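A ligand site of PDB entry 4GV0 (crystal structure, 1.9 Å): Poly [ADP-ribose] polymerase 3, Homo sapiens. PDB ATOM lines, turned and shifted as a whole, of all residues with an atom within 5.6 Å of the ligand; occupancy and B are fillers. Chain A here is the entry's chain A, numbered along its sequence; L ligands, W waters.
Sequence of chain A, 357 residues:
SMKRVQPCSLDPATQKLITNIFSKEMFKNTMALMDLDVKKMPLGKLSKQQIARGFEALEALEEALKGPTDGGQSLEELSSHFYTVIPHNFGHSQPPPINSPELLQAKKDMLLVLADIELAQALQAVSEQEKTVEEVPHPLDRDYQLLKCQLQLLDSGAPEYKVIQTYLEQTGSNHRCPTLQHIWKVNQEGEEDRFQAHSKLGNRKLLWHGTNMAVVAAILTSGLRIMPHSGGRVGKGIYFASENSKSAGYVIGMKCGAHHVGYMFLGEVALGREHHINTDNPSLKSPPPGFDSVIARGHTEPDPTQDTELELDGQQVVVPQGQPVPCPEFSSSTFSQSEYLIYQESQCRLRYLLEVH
O of Trp 208 lies within hydrogen-bond range of OG of Ser 247 (3.3 Å). The side-chain carboxylate of Asp 116 lies within salt-bridge range of the guanidinium group of Arg 225, 2.9 Å away. A ring nitrogen (ND1) of His 209 sits at hydrogen-bond distance from the backbone carbonyl oxygen (O) of Tyr 239 (2.6 Å). The side-chain carboxylate (OE2) of Glu 339 is in salt-bridge range of the side-chain amino group (NZ) of Lys 246, 2.6 Å away. The backbone NH (N) of Trp 208 lies within hydrogen-bond range of the backbone carbonyl oxygen (O) of Ala 241 (2.8 Å). The backbone NH of Met 227 sits at hydrogen-bond distance from the side-chain hydroxyl of Ser 230, 2.8 Å away.
OG of Ser 247 lies within hydrogen-bond range of O2 of the ligand (2.7 Å). The backbone NH of Gly 210 sits at hydrogen-bond distance from an oxygen (O2) of the ligand, at 2.8 Å. The backbone carbonyl oxygen (O) of Gly 210 sits at hydrogen-bond distance from a nitrogen (N4) of the ligand (2.8 Å).
Water W1 bridges an oxygen (O1) of the ligand and the side-chain amide nitrogen of Asn 212. Water W3 lies within hydrogen-bond range of N1 of the ligand (2.7 Å) and OG of Ser 230 (3.1 Å).
Asp 109 touches the ligand (CG to C7, 3.6 Å). Leu 112 touches the ligand. Asp 116 touches the ligand (OD2 to C2, 3.3 Å). Trp 208 touches the ligand (O to O2, 3.96 Å). His 209 touches the ligand. Thr 211 touches the ligand. SD of Met 227 touches C4 of the ligand, at 3.999 Å. Tyr 239 touches the ligand. Phe 240 touches the ligand. Tyr 250 touches the ligand. Glu 339 touches the ligand (OE1 to C14, 3.5 Å). 13 residues have an atom within 4 Å of the ligand: Asp 109, Leu 112, Asp 116, Trp 208, His 209, Gly 210, Thr 211, Met 227, Tyr 239, Phe 240, Ser 247, Tyr 250 and Glu 339.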
ATOM      1  N   ASP A 109       6.815 -11.889 -27.866  1.00  0.00           N
ATOM      2  CA  ASP A 109       7.706 -10.739 -28.019  1.00  0.00           C
ATOM      3  C   ASP A 109       9.162 -11.141 -28.349  1.00  0.00           C
ATOM      4  O   ASP A 109       9.807 -10.524 -29.208  1.00  0.00           O
ATOM      5  CB  ASP A 109       7.642  -9.859 -26.800  1.00  0.00           C
ATOM      6  CG  ASP A 109       6.348  -9.042 -26.744  1.00  0.00           C
ATOM      7  OD1 ASP A 109       5.505  -9.135 -27.698  1.00  0.00           O
ATOM      8  OD2 ASP A 109       6.161  -8.281 -25.776  1.00  0.00           O
ATOM      9  N   LEU A 112       9.142 -12.099 -32.022  1.00  0.00           N
ATOM     10  CA  LEU A 112       9.118 -10.882 -32.840  1.00  0.00           C
ATOM     11  C   LEU A 112      10.508 -10.227 -32.943  1.00  0.00           C
ATOM     12  O   LEU A 112      10.929  -9.794 -34.051  1.00  0.00           O
ATOM     13  CB  LEU A 112       8.123  -9.870 -32.275  1.00  0.00           C
ATOM     14  CG  LEU A 112       6.629 -10.240 -32.417  1.00  0.00           C
ATOM     15  CD1 LEU A 112       5.737  -9.281 -31.657  1.00  0.00           C
ATOM     16  CD2 LEU A 112       6.273 -10.239 -33.922  1.00  0.00           C
ATOM     17  N   VAL A 113      11.242 -10.210 -31.816  1.00  0.00           N
ATOM     18  CA  VAL A 113      12.675  -9.836 -31.860  1.00  0.00           C
ATOM     19  C   VAL A 113      13.491 -10.779 -32.754  1.00  0.00           C
ATOM     20  O   VAL A 113      14.239 -10.334 -33.613  1.00  0.00           O
ATOM     21  CB  VAL A 113      13.306  -9.725 -30.413  1.00  0.00           C
ATOM     22  CG1 VAL A 113      14.848  -9.411 -30.484  1.00  0.00           C
ATOM     23  CG2 VAL A 113      12.539  -8.643 -29.551  1.00  0.00           C
ATOM     24  N   ASP A 116      13.108 -10.218 -36.422  1.00  0.00           N
ATOM     25  CA  ASP A 116      13.859  -9.097 -36.921  1.00  0.00           C
ATOM     26  C   ASP A 116      15.354  -9.372 -37.000  1.00  0.00           C
ATOM     27  O   ASP A 116      16.023  -8.732 -37.791  1.00  0.00           O
ATOM     28  CB  ASP A 116      13.581  -7.807 -36.136  1.00  0.00           C
ATOM     29  CG  ASP A 116      12.216  -7.189 -36.515  1.00  0.00           C
ATOM     30  OD1 ASP A 116      11.541  -7.712 -37.472  1.00  0.00           O
ATOM     31  OD2 ASP A 116      11.863  -6.137 -35.915  1.00  0.00           O
ATOM     32  N   TRP A 208       8.526   9.225 -28.532  1.00  0.00           N
ATOM     33  CA  TRP A 208       9.621   8.303 -28.333  1.00  0.00           C
ATOM     34  C   TRP A 208       9.192   6.874 -28.643  1.00  0.00           C
ATOM     35  O   TRP A 208       8.035   6.464 -28.374  1.00  0.00           O
ATOM     36  CB  TRP A 208      10.136   8.374 -26.897  1.00  0.00           C
ATOM     37  CG  TRP A 208      10.710   9.688 -26.545  1.00  0.00           C
ATOM     38  CD1 TRP A 208      10.150  10.657 -25.772  1.00  0.00           C
ATOM     39  CD2 TRP A 208      12.010  10.167 -26.922  1.00  0.00           C
ATOM     40  NE1 TRP A 208      11.028  11.745 -25.669  1.00  0.00           N
ATOM     41  CE2 TRP A 208      12.155  11.475 -26.382  1.00  0.00           C
ATOM     42  CE3 TRP A 208      13.025   9.656 -27.722  1.00  0.00           C
ATOM     43  CZ2 TRP A 208      13.289  12.246 -26.597  1.00  0.00           C
ATOM     44  CZ3 TRP A 208      14.160  10.417 -27.948  1.00  0.00           C
ATOM     45  CH2 TRP A 208      14.290  11.708 -27.369  1.00  0.00           C
ATOM     46  N   HIS A 209      10.113   6.117 -29.214  1.00  0.00           N
ATOM     47  CA  HIS A 209       9.941   4.668 -29.353  1.00  0.00           C
ATOM     48  C   HIS A 209      11.279   4.007 -29.080  1.00  0.00           C
ATOM     49  O   HIS A 209      12.229   4.163 -29.860  1.00  0.00           O
ATOM     50  CB  HIS A 209       9.363   4.319 -30.710  1.00  0.00           C
ATOM     51  CG  HIS A 209       9.052   2.869 -30.904  1.00  0.00           C
ATOM     52  ND1 HIS A 209       7.841   2.313 -30.544  1.00  0.00           N
ATOM     53  CD2 HIS A 209       9.800   1.863 -31.419  1.00  0.00           C
ATOM     54  CE1 HIS A 209       7.853   1.017 -30.852  1.00  0.00           C
ATOM     55  NE2 HIS A 209       9.040   0.707 -31.341  1.00  0.00           N
ATOM     56  N   GLY A 210      11.407   3.348 -27.919  1.00  0.00           N
ATOM     57  CA  GLY A 210      12.602   2.548 -27.610  1.00  0.00           C
ATOM     58  C   GLY A 210      12.502   1.092 -28.034  1.00  0.00           C
ATOM     59  O   GLY A 210      11.431   0.489 -27.917  1.00  0.00           O
ATOM     60  N   THR A 211      13.647   0.481 -28.416  1.00  0.00           N
ATOM     61  CA  THR A 211      13.667  -0.936 -28.762  1.00  0.00           C
ATOM     62  C   THR A 211      15.006  -1.537 -28.428  1.00  0.00           C
ATOM     63  O   THR A 211      15.937  -0.808 -28.092  1.00  0.00           O
ATOM     64  CB  THR A 211      13.469  -1.148 -30.301  1.00  0.00           C
ATOM     65  OG1 THR A 211      14.600  -0.632 -30.998  1.00  0.00           O
ATOM     66  CG2 THR A 211      12.225  -0.462 -30.817  1.00  0.00           C
ATOM     67  N   ASN A 212      15.077  -2.859 -28.514  1.00  0.00           N
ATOM     68  CA  ASN A 212      16.328  -3.631 -28.567  1.00  0.00           C
ATOM     69  C   ASN A 212      17.214  -3.133 -29.714  1.00  0.00           C
ATOM     70  O   ASN A 212      16.698  -2.836 -30.815  1.00  0.00           O
ATOM     71  CB  ASN A 212      16.027  -5.116 -28.979  1.00  0.00           C
ATOM     72  CG  ASN A 212      15.779  -6.064 -27.814  1.00  0.00           C
ATOM     73  OD1 ASN A 212      16.723  -6.697 -27.303  1.00  0.00           O
ATOM     74  ND2 ASN A 212      14.530  -6.265 -27.462  1.00  0.00           N
ATOM     75  N   VAL A 215      16.657  -4.895 -33.193  1.00  0.00           N
ATOM     76  CA  VAL A 215      15.571  -4.675 -34.133  1.00  0.00           C
ATOM     77  C   VAL A 215      15.729  -3.352 -34.919  1.00  0.00           C
ATOM     78  O   VAL A 215      14.865  -2.996 -35.734  1.00  0.00           O
ATOM     79  CB  VAL A 215      14.188  -4.849 -33.457  1.00  0.00           C
ATOM     80  CG1 VAL A 215      14.134  -6.136 -32.594  1.00  0.00           C
ATOM     81  CG2 VAL A 215      13.853  -3.684 -32.671  1.00  0.00           C
ATOM     82  N   ARG A 225       6.159  -1.414 -37.094  1.00  0.00           N
ATOM     83  CA  ARG A 225       5.193  -2.365 -37.649  1.00  0.00           C
ATOM     84  C   ARG A 225       4.284  -2.896 -36.543  1.00  0.00           C
ATOM     85  O   ARG A 225       4.645  -2.896 -35.347  1.00  0.00           O
ATOM     86  CB  ARG A 225       5.970  -3.536 -38.310  1.00  0.00           C
ATOM     87  CG  ARG A 225       6.680  -3.126 -39.613  1.00  0.00           C
ATOM     88  CD  ARG A 225       7.972  -3.874 -39.862  1.00  0.00           C
ATOM     89  NE  ARG A 225       8.911  -3.547 -38.808  1.00  0.00           N
ATOM     90  CZ  ARG A 225       9.730  -4.409 -38.204  1.00  0.00           C
ATOM     91  NH1 ARG A 225       9.835  -5.689 -38.593  1.00  0.00           N
ATOM     92  NH2 ARG A 225      10.448  -3.972 -37.198  1.00  0.00           N
ATOM     93  N   MET A 227       2.506  -6.529 -35.892  1.00  0.00           N
ATOM     94  CA  MET A 227       2.392  -7.932 -36.378  1.00  0.00           C
ATOM     95  C   MET A 227       1.268  -8.703 -35.740  1.00  0.00           C
ATOM     96  O   MET A 227       0.699  -8.304 -34.720  1.00  0.00           O
ATOM     97  CB  MET A 227       3.690  -8.747 -36.344  1.00  0.00           C
ATOM     98  CG  MET A 227       4.882  -8.165 -35.687  1.00  0.00           C
ATOM     99  SD  MET A 227       5.460  -6.634 -36.312  1.00  0.00           S
ATOM    100  CE  MET A 227       6.139  -7.211 -37.895  1.00  0.00           C
ATOM    101  N   SER A 230       1.632  -9.061 -32.146  1.00  0.00           N
ATOM    102  CA  SER A 230       1.920  -7.850 -31.315  1.00  0.00           C
ATOM    103  C   SER A 230       0.875  -7.669 -30.208  1.00  0.00           C
ATOM    104  O   SER A 230      -0.268  -7.958 -30.400  1.00  0.00           O
ATOM    105  CB  SER A 230       1.983  -6.588 -32.158  1.00  0.00           C
ATOM    106  OG  SER A 230       2.950  -6.696 -33.152  1.00  0.00           O
ATOM    107  N   TYR A 239       3.403   1.205 -29.978  1.00  0.00           N
ATOM    108  CA  TYR A 239       3.469   1.922 -28.727  1.00  0.00           C
ATOM    109  C   TYR A 239       4.525   3.014 -28.765  1.00  0.00           C
ATOM    110  O   TYR A 239       5.660   2.807 -29.198  1.00  0.00           O
ATOM    111  CB  TYR A 239       3.844   0.960 -27.615  1.00  0.00           C
ATOM    112  CG  TYR A 239       2.783  -0.029 -27.258  1.00  0.00           C
ATOM    113  CD1 TYR A 239       2.020   0.138 -26.099  1.00  0.00           C
ATOM    114  CD2 TYR A 239       2.515  -1.118 -28.067  1.00  0.00           C
ATOM    115  CE1 TYR A 239       1.037  -0.752 -25.738  1.00  0.00           C
ATOM    116  CE2 TYR A 239       1.512  -2.022 -27.733  1.00  0.00           C
ATOM    117  CZ  TYR A 239       0.772  -1.821 -26.570  1.00  0.00           C
ATOM    118  OH  TYR A 239      -0.244  -2.685 -26.235  1.00  0.00           O
ATOM    119  N   PHE A 240       4.132   4.183 -28.302  1.00  0.00           N
ATOM    120  CA  PHE A 240       5.039   5.307 -28.141  1.00  0.00           C
ATOM    121  C   PHE A 240       4.895   5.887 -26.729  1.00  0.00           C
ATOM    122  O   PHE A 240       3.850   5.717 -26.033  1.00  0.00           O
ATOM    123  CB  PHE A 240       4.685   6.415 -29.130  1.00  0.00           C
ATOM    124  CG  PHE A 240       4.771   6.022 -30.583  1.00  0.00           C
ATOM    125  CD1 PHE A 240       5.946   6.265 -31.309  1.00  0.00           C
ATOM    126  CD2 PHE A 240       3.716   5.379 -31.207  1.00  0.00           C
ATOM    127  CE1 PHE A 240       6.052   5.911 -32.634  1.00  0.00           C
ATOM    128  CE2 PHE A 240       3.779   5.038 -32.541  1.00  0.00           C
ATOM    129  CZ  PHE A 240       4.947   5.291 -33.285  1.00  0.00           C
ATOM    130  N   ALA A 241       5.862   6.714 -26.357  1.00  0.00           N
ATOM    131  CA  ALA A 241       5.740   7.479 -25.126  1.00  0.00           C
ATOM    132  C   ALA A 241       6.114   8.950 -25.350  1.00  0.00           C
ATOM    133  O   ALA A 241       7.011   9.260 -26.153  1.00  0.00           O
ATOM    134  CB  ALA A 241       6.657   6.862 -24.056  1.00  0.00           C
ATOM    135  N   LYS A 246      10.004   6.481 -20.059  1.00  0.00           N
ATOM    136  CA  LYS A 246       9.175   5.326 -20.348  1.00  0.00           C
ATOM    137  C   LYS A 246       9.747   4.482 -21.521  1.00  0.00           C
ATOM    138  O   LYS A 246       9.894   3.279 -21.390  1.00  0.00           O
ATOM    139  CB  LYS A 246       7.701   5.772 -20.613  1.00  0.00           C
ATOM    140  CG  LYS A 246       6.740   4.616 -21.004  1.00  0.00           C
ATOM    141  CD  LYS A 246       6.443   3.678 -19.826  1.00  0.00           C
ATOM    142  CE  LYS A 246       5.356   2.633 -20.041  1.00  0.00           C
ATOM    143  NZ  LYS A 246       3.899   2.978 -19.483  1.00  0.00           N
ATOM    144  N   SER A 247       9.997   5.088 -22.693  1.00  0.00           N
ATOM    145  CA  SER A 247      10.579   4.398 -23.816  1.00  0.00           C
ATOM    146  C   SER A 247      11.977   3.802 -23.551  1.00  0.00           C
ATOM    147  O   SER A 247      12.349   2.737 -24.073  1.00  0.00           O
ATOM    148  CB  SER A 247      10.665   5.342 -25.029  1.00  0.00           C
ATOM    149  OG  SER A 247       9.368   5.441 -25.583  1.00  0.00           O
ATOM    150  N   TYR A 250      12.627   0.188 -22.557  1.00  0.00           N
ATOM    151  CA  TYR A 250      12.631  -0.854 -23.563  1.00  0.00           C
ATOM    152  C   TYR A 250      13.921  -0.934 -24.286  1.00  0.00           C
ATOM    153  O   TYR A 250      14.096  -1.820 -25.119  1.00  0.00           O
ATOM    154  CB  TYR A 250      11.476  -0.634 -24.531  1.00  0.00           C
ATOM    155  CG  TYR A 250      10.188  -0.753 -23.822  1.00  0.00           C
ATOM    156  CD1 TYR A 250       9.617  -2.008 -23.645  1.00  0.00           C
ATOM    157  CD2 TYR A 250       9.571   0.346 -23.262  1.00  0.00           C
ATOM    158  CE1 TYR A 250       8.442  -2.169 -22.949  1.00  0.00           C
ATOM    159  CE2 TYR A 250       8.380   0.210 -22.579  1.00  0.00           C
ATOM    160  CZ  TYR A 250       7.818  -1.064 -22.432  1.00  0.00           C
ATOM    161  OH  TYR A 250       6.643  -1.225 -21.736  1.00  0.00           O
ATOM    162  N   SER A 338       2.225   7.908 -19.759  1.00  0.00           N
ATOM    163  CA  SER A 338       1.304   7.669 -20.917  1.00  0.00           C
ATOM    164  C   SER A 338       1.888   6.733 -21.951  1.00  0.00           C
ATOM    165  O   SER A 338       3.139   6.727 -22.191  1.00  0.00           O
ATOM    166  CB  SER A 338       0.908   9.000 -21.572  1.00  0.00           C
ATOM    167  OG  SER A 338       0.146   9.866 -20.709  1.00  0.00           O
ATOM    168  N   GLU A 339       1.008   5.946 -22.599  1.00  0.00           N
ATOM    169  CA  GLU A 339       1.353   5.129 -23.745  1.00  0.00           C
ATOM    170  C   GLU A 339       0.408   5.592 -24.841  1.00  0.00           C
ATOM    171  O   GLU A 339      -0.836   5.598 -24.646  1.00  0.00           O
ATOM    172  CB  GLU A 339       1.178   3.613 -23.455  1.00  0.00           C
ATOM    173  CG  GLU A 339       1.946   3.170 -22.155  1.00  0.00           C
ATOM    174  CD  GLU A 339       2.016   1.698 -21.919  1.00  0.00           C
ATOM    175  OE1 GLU A 339       1.645   0.901 -22.794  1.00  0.00           O
ATOM    176  OE2 GLU A 339       2.453   1.310 -20.812  1.00  0.00           O
HETATM  177  C1  LIG L   1      10.129  -6.204 -31.759  1.00  0.00           C
HETATM  178  C2  LIG L   1      10.151  -6.427 -33.129  1.00  0.00           C
HETATM  179  C3  LIG L   1       8.956  -6.330 -33.794  1.00  0.00           C
HETATM  180  C4  LIG L   1       7.777  -6.023 -33.110  1.00  0.00           C
HETATM  181  N1  LIG L   1       7.778  -5.822 -31.810  1.00  0.00           N
HETATM  182  C5  LIG L   1       8.936  -5.876 -31.112  1.00  0.00           C
HETATM  183  C6  LIG L   1       8.914  -5.676 -29.613  1.00  0.00           C
HETATM  184  C7  LIG L   1       8.003  -6.786 -29.074  1.00  0.00           C
HETATM  185  N2  LIG L   1       8.328  -4.380 -29.253  1.00  0.00           N
HETATM  186  C8  LIG L   1       9.091  -3.296 -29.200  1.00  0.00           C
HETATM  187  O1  LIG L   1      10.283  -3.332 -29.434  1.00  0.00           O
HETATM  188  C9  LIG L   1       8.414  -1.989 -28.771  1.00  0.00           C
HETATM  189  C10 LIG L   1       8.967  -1.633 -27.395  1.00  0.00           C
HETATM  190  C11 LIG L   1       8.281  -0.475 -26.765  1.00  0.00           C
HETATM  191  N3  LIG L   1       7.146  -0.601 -26.027  1.00  0.00           N
HETATM  192  C12 LIG L   1       6.599   0.532 -25.503  1.00  0.00           C
HETATM  193  C13 LIG L   1       5.444   0.414 -24.693  1.00  0.00           C
HETATM  194  C14 LIG L   1       4.836   1.525 -24.114  1.00  0.00           C
HETATM  195  C15 LIG L   1       5.426   2.780 -24.352  1.00  0.00           C
HETATM  196  C16 LIG L   1       6.611   2.889 -25.114  1.00  0.00           C
HETATM  197  C17 LIG L   1       7.218   1.782 -25.668  1.00  0.00           C
HETATM  198  C18 LIG L   1       8.369   1.921 -26.433  1.00  0.00           C
HETATM  199  O2  LIG L   1       8.951   3.031 -26.619  1.00  0.00           O
HETATM  200  N4  LIG L   1       8.868   0.752 -26.954  1.00  0.00           N
HETATM  201  O   HOH W   1      12.559  -4.458 -28.814  1.00  0.00           O
HETATM  202  O   HOH W   2       5.920  -3.032 -26.207  1.00  0.00           O
HETATM  203  O   HOH W   3       5.110  -5.382 -31.387  1.00  0.00           O
HETATM  204  O   HOH W   4       5.279  -3.486 -28.841  1.00  0.00           O
